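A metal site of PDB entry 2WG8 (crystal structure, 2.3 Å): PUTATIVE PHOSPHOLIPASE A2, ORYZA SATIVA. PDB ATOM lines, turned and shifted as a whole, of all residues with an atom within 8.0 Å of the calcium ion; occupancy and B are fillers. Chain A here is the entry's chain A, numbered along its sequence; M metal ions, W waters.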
ATOM      1  N   LEU A  33      -1.783 -11.126  24.306  1.00  0.00           N
ATOM      2  CA  LEU A  33      -0.850 -11.846  25.170  1.00  0.00           C
ATOM      3  C   LEU A  33       0.354 -10.999  25.581  1.00  0.00           C
ATOM      4  O   LEU A  33       0.974 -10.354  24.746  1.00  0.00           O
ATOM      5  CB  LEU A  33      -0.379 -13.137  24.478  1.00  0.00           C
ATOM      6  CG  LEU A  33       0.394 -14.195  25.287  1.00  0.00           C
ATOM      7  CD1 LEU A  33       0.146 -15.559  24.698  1.00  0.00           C
ATOM      8  CD2 LEU A  33       1.885 -13.899  25.330  1.00  0.00           C
ATOM      9  N   ARG A  34       0.647 -11.017  26.881  1.00  0.00           N
ATOM     10  CA  ARG A  34       1.874 -10.479  27.433  1.00  0.00           C
ATOM     11  C   ARG A  34       2.297 -11.442  28.514  1.00  0.00           C
ATOM     12  O   ARG A  34       1.583 -11.642  29.492  1.00  0.00           O
ATOM     13  CB  ARG A  34       1.692  -9.078  28.011  1.00  0.00           C
ATOM     14  CG  ARG A  34       1.742  -8.015  26.962  1.00  0.00           C
ATOM     15  CD  ARG A  34       1.502  -6.636  27.528  1.00  0.00           C
ATOM     16  NE  ARG A  34       1.496  -5.692  26.423  1.00  0.00           N
ATOM     17  CZ  ARG A  34       1.288  -4.392  26.528  1.00  0.00           C
ATOM     18  NH1 ARG A  34       1.063  -3.815  27.709  1.00  0.00           N
ATOM     19  NH2 ARG A  34       1.312  -3.654  25.440  1.00  0.00           N
ATOM     20  N   TYR A  35       3.459 -12.046  28.332  1.00  0.00           N
ATOM     21  CA  TYR A  35       3.920 -13.099  29.214  1.00  0.00           C
ATOM     22  C   TYR A  35       5.407 -12.872  29.460  1.00  0.00           C
ATOM     23  O   TYR A  35       6.192 -12.748  28.512  1.00  0.00           O
ATOM     24  CB  TYR A  35       3.659 -14.452  28.554  1.00  0.00           C
ATOM     25  CG  TYR A  35       4.151 -15.678  29.304  1.00  0.00           C
ATOM     26  CD1 TYR A  35       3.245 -16.553  29.917  1.00  0.00           C
ATOM     27  CD2 TYR A  35       5.516 -15.974  29.371  1.00  0.00           C
ATOM     28  CE1 TYR A  35       3.697 -17.695  30.604  1.00  0.00           C
ATOM     29  CE2 TYR A  35       5.966 -17.081  30.045  1.00  0.00           C
ATOM     30  CZ  TYR A  35       5.058 -17.938  30.658  1.00  0.00           C
ATOM     31  OH  TYR A  35       5.565 -19.029  31.322  1.00  0.00           O
ATOM     32  N   LYS A  37       8.783 -10.917  30.477  1.00  0.00           N
ATOM     33  CA  LYS A  37       9.236  -9.612  30.049  1.00  0.00           C
ATOM     34  C   LYS A  37       9.302  -9.492  28.518  1.00  0.00           C
ATOM     35  O   LYS A  37       9.393  -8.381  27.991  1.00  0.00           O
ATOM     36  CB  LYS A  37      10.617  -9.305  30.638  1.00  0.00           C
ATOM     37  CG  LYS A  37      10.626  -9.000  32.137  1.00  0.00           C
ATOM     38  CD  LYS A  37      12.071  -8.986  32.636  1.00  0.00           C
ATOM     39  CE  LYS A  37      12.152  -9.173  34.145  1.00  0.00           C
ATOM     40  NZ  LYS A  37      13.573  -9.328  34.560  1.00  0.00           N
ATOM     41  N   TYR A  38       9.243 -10.640  27.827  1.00  0.00           N
ATOM     42  CA  TYR A  38       9.559 -10.720  26.391  1.00  0.00           C
ATOM     43  C   TYR A  38       8.470 -11.248  25.465  1.00  0.00           C
ATOM     44  O   TYR A  38       8.467 -10.882  24.293  1.00  0.00           O
ATOM     45  CB  TYR A  38      10.844 -11.514  26.147  1.00  0.00           C
ATOM     46  CG  TYR A  38      12.058 -10.821  26.703  1.00  0.00           C
ATOM     47  CD1 TYR A  38      12.490 -11.076  28.012  1.00  0.00           C
ATOM     48  CD2 TYR A  38      12.750  -9.887  25.945  1.00  0.00           C
ATOM     49  CE1 TYR A  38      13.591 -10.439  28.538  1.00  0.00           C
ATOM     50  CE2 TYR A  38      13.879  -9.241  26.466  1.00  0.00           C
ATOM     51  CZ  TYR A  38      14.285  -9.521  27.765  1.00  0.00           C
ATOM     52  OH  TYR A  38      15.386  -8.884  28.291  1.00  0.00           O
ATOM     53  N   CYS A  39       7.558 -12.080  25.980  1.00  0.00           N
ATOM     54  CA  CYS A  39       6.591 -12.771  25.106  1.00  0.00           C
ATOM     55  C   CYS A  39       5.359 -11.938  24.907  1.00  0.00           C
ATOM     56  O   CYS A  39       4.563 -11.727  25.836  1.00  0.00           O
ATOM     57  CB  CYS A  39       6.164 -14.141  25.668  1.00  0.00           C
ATOM     58  SG  CYS A  39       7.415 -15.378  25.870  1.00  0.00           S
ATOM     59  N   GLY A  40       5.175 -11.472  23.677  1.00  0.00           N
ATOM     60  CA  GLY A  40       4.040 -10.661  23.335  1.00  0.00           C
ATOM     61  C   GLY A  40       4.411  -9.792  22.158  1.00  0.00           C
ATOM     62  O   GLY A  40       5.593  -9.488  21.949  1.00  0.00           O
ATOM     63  N   ILE A  41       3.387  -9.379  21.414  1.00  0.00           N
ATOM     64  CA  ILE A  41       3.535  -8.576  20.222  1.00  0.00           C
ATOM     65  C   ILE A  41       3.934  -7.146  20.602  1.00  0.00           C
ATOM     66  O   ILE A  41       3.255  -6.503  21.409  1.00  0.00           O
ATOM     67  CB  ILE A  41       2.221  -8.587  19.397  1.00  0.00           C
ATOM     68  CG1 ILE A  41       1.999  -9.971  18.760  1.00  0.00           C
ATOM     69  CG2 ILE A  41       2.219  -7.476  18.333  1.00  0.00           C
ATOM     70  CD1 ILE A  41       0.553 -10.295  18.371  1.00  0.00           C
ATOM     71  N   LEU A  42       5.038  -6.666  20.017  1.00  0.00           N
ATOM     72  CA  LEU A  42       5.573  -5.326  20.318  1.00  0.00           C
ATOM     73  C   LEU A  42       5.693  -5.069  21.822  1.00  0.00           C
ATOM     74  O   LEU A  42       5.355  -3.981  22.323  1.00  0.00           O
ATOM     75  CB  LEU A  42       4.778  -4.220  19.588  1.00  0.00           C
ATOM     76  CG  LEU A  42       4.873  -4.190  18.049  1.00  0.00           C
ATOM     77  CD1 LEU A  42       4.018  -3.075  17.472  1.00  0.00           C
ATOM     78  CD2 LEU A  42       6.311  -4.042  17.575  1.00  0.00           C
ATOM     79  N   TYR A  43       6.201  -6.073  22.523  1.00  0.00           N
ATOM     80  CA  TYR A  43       6.343  -6.061  23.957  1.00  0.00           C
ATOM     81  C   TYR A  43       7.661  -6.761  24.228  1.00  0.00           C
ATOM     82  O   TYR A  43       7.826  -7.915  23.891  1.00  0.00           O
ATOM     83  CB  TYR A  43       5.176  -6.804  24.614  1.00  0.00           C
ATOM     84  CG  TYR A  43       5.400  -7.087  26.072  1.00  0.00           C
ATOM     85  CD1 TYR A  43       5.295  -6.065  27.012  1.00  0.00           C
ATOM     86  CD2 TYR A  43       5.733  -8.373  26.507  1.00  0.00           C
ATOM     87  CE1 TYR A  43       5.523  -6.310  28.357  1.00  0.00           C
ATOM     88  CE2 TYR A  43       5.975  -8.634  27.846  1.00  0.00           C
ATOM     89  CZ  TYR A  43       5.853  -7.601  28.770  1.00  0.00           C
ATOM     90  OH  TYR A  43       6.089  -7.834  30.103  1.00  0.00           O
ATOM     91  N   SER A  44       8.594  -6.066  24.859  1.00  0.00           N
ATOM     92  CA  SER A  44       9.917  -6.606  25.030  1.00  0.00           C
ATOM     93  C   SER A  44      10.563  -6.116  26.317  1.00  0.00           C
ATOM     94  O   SER A  44      10.205  -5.042  26.839  1.00  0.00           O
ATOM     95  CB  SER A  44      10.788  -6.213  23.833  1.00  0.00           C
ATOM     96  OG  SER A  44      11.692  -7.248  23.523  1.00  0.00           O
ATOM     97  N   GLY A  45      11.499  -6.897  26.839  1.00  0.00           N
ATOM     98  CA  GLY A  45      12.239  -6.512  28.023  1.00  0.00           C
ATOM     99  C   GLY A  45      13.283  -5.436  27.744  1.00  0.00           C
ATOM    100  O   GLY A  45      13.876  -5.372  26.655  1.00  0.00           O
ATOM    101  N   ASP A  56       9.968 -17.507  28.419  1.00  0.00           N
ATOM    102  CA  ASP A  56      10.352 -16.101  28.287  1.00  0.00           C
ATOM    103  C   ASP A  56      11.690 -15.922  27.602  1.00  0.00           C
ATOM    104  O   ASP A  56      11.859 -14.994  26.811  1.00  0.00           O
ATOM    105  CB  ASP A  56      10.329 -15.383  29.647  1.00  0.00           C
ATOM    106  CG  ASP A  56      10.171 -13.875  29.500  1.00  0.00           C
ATOM    107  OD1 ASP A  56       9.513 -13.446  28.537  1.00  0.00           O
ATOM    108  OD2 ASP A  56      10.682 -13.113  30.348  1.00  0.00           O
ATOM    109  N   CYS A  59      11.480 -16.218  23.887  1.00  0.00           N
ATOM    110  CA  CYS A  59      10.947 -14.966  23.362  1.00  0.00           C
ATOM    111  C   CYS A  59      11.966 -13.835  23.317  1.00  0.00           C
ATOM    112  O   CYS A  59      11.932 -13.004  22.433  1.00  0.00           O
ATOM    113  CB  CYS A  59       9.727 -14.517  24.159  1.00  0.00           C
ATOM    114  SG  CYS A  59       8.251 -15.551  24.009  1.00  0.00           S
ATOM    115  N   MET A  60      12.875 -13.812  24.287  1.00  0.00           N
ATOM    116  CA  MET A  60      13.978 -12.849  24.327  1.00  0.00           C
ATOM    117  C   MET A  60      14.942 -13.011  23.155  1.00  0.00           C
ATOM    118  O   MET A  60      15.343 -12.031  22.522  1.00  0.00           O
ATOM    119  CB  MET A  60      14.747 -13.004  25.631  1.00  0.00           C
ATOM    120  CG  MET A  60      16.002 -12.173  25.726  1.00  0.00           C
ATOM    121  SD  MET A  60      16.878 -12.585  27.241  1.00  0.00           S
ATOM    122  CE  MET A  60      17.990 -11.178  27.422  1.00  0.00           C
ATOM    123  N   HIS A  62      14.204 -14.548  20.320  1.00  0.00           N
ATOM    124  CA  HIS A  62      13.431 -14.234  19.120  1.00  0.00           C
ATOM    125  C   HIS A  62      13.356 -12.728  18.899  1.00  0.00           C
ATOM    126  O   HIS A  62      13.534 -12.266  17.790  1.00  0.00           O
ATOM    127  CB  HIS A  62      12.025 -14.833  19.200  1.00  0.00           C
ATOM    128  CG  HIS A  62      11.136 -14.456  18.066  1.00  0.00           C
ATOM    129  ND1 HIS A  62      10.317 -13.354  18.100  1.00  0.00           N
ATOM    130  CD2 HIS A  62      10.967 -15.015  16.848  1.00  0.00           C
ATOM    131  CE1 HIS A  62       9.658 -13.257  16.957  1.00  0.00           C
ATOM    132  NE2 HIS A  62      10.035 -14.259  16.184  1.00  0.00           N
ATOM    133  N   ASP A  63      13.126 -11.970  19.979  1.00  0.00           N
ATOM    134  CA  ASP A  63      12.950 -10.528  19.892  1.00  0.00           C
ATOM    135  C   ASP A  63      14.207  -9.839  19.373  1.00  0.00           C
ATOM    136  O   ASP A  63      14.125  -8.949  18.516  1.00  0.00           O
ATOM    137  CB  ASP A  63      12.581  -9.947  21.262  1.00  0.00           C
ATOM    138  CG  ASP A  63      11.124 -10.098  21.587  1.00  0.00           C
ATOM    139  OD1 ASP A  63      10.363 -10.574  20.725  1.00  0.00           O
ATOM    140  OD2 ASP A  63      10.715  -9.723  22.708  1.00  0.00           O
ATOM    141  N   HIS A  64      15.350 -10.242  19.912  1.00  0.00           N
ATOM    142  CA  HIS A  64      16.654  -9.725  19.483  1.00  0.00           C
ATOM    143  C   HIS A  64      17.030 -10.177  18.075  1.00  0.00           C
ATOM    144  O   HIS A  64      17.662  -9.423  17.349  1.00  0.00           O
ATOM    145  CB  HIS A  64      17.741 -10.150  20.479  1.00  0.00           C
ATOM    146  CG  HIS A  64      17.704  -9.403  21.768  1.00  0.00           C
ATOM    147  ND1 HIS A  64      17.073  -9.906  22.898  1.00  0.00           N
ATOM    148  CD2 HIS A  64      18.195  -8.196  22.112  1.00  0.00           C
ATOM    149  CE1 HIS A  64      17.183  -9.028  23.874  1.00  0.00           C
ATOM    150  NE2 HIS A  64      17.857  -7.981  23.437  1.00  0.00           N
HETATM  151 CA    CA M   1       7.992  -9.514  22.364  1.00  0.00          CA
HETATM  152  O   HOH W   1       8.029  -7.686  20.381  1.00  0.00           O
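The calcium ion is bound by the backbone carbonyl oxygen of Tyr 43, the backbone carbonyl oxygen of Tyr 38, the backbone carbonyl oxygen of Gly 40, water W1 and the side-chain carboxylate of Asp 63. Slightly farther from the calcium ion lies OD1 of Asp 63 (3.1 Å).
The side-chain carboxylate (OD1) of Asp 56 sits at hydrogen-bond distance from the backbone NH (N) of Tyr 38 (2.9 Å). The side-chain carboxylate (OD2) of Asp 63 sits close to the side-chain hydroxyl (OG) of Ser 44 (2.8 Å). SG of Cys 39 forms a disulfide with SG of Cys 59 (2.0 Å).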
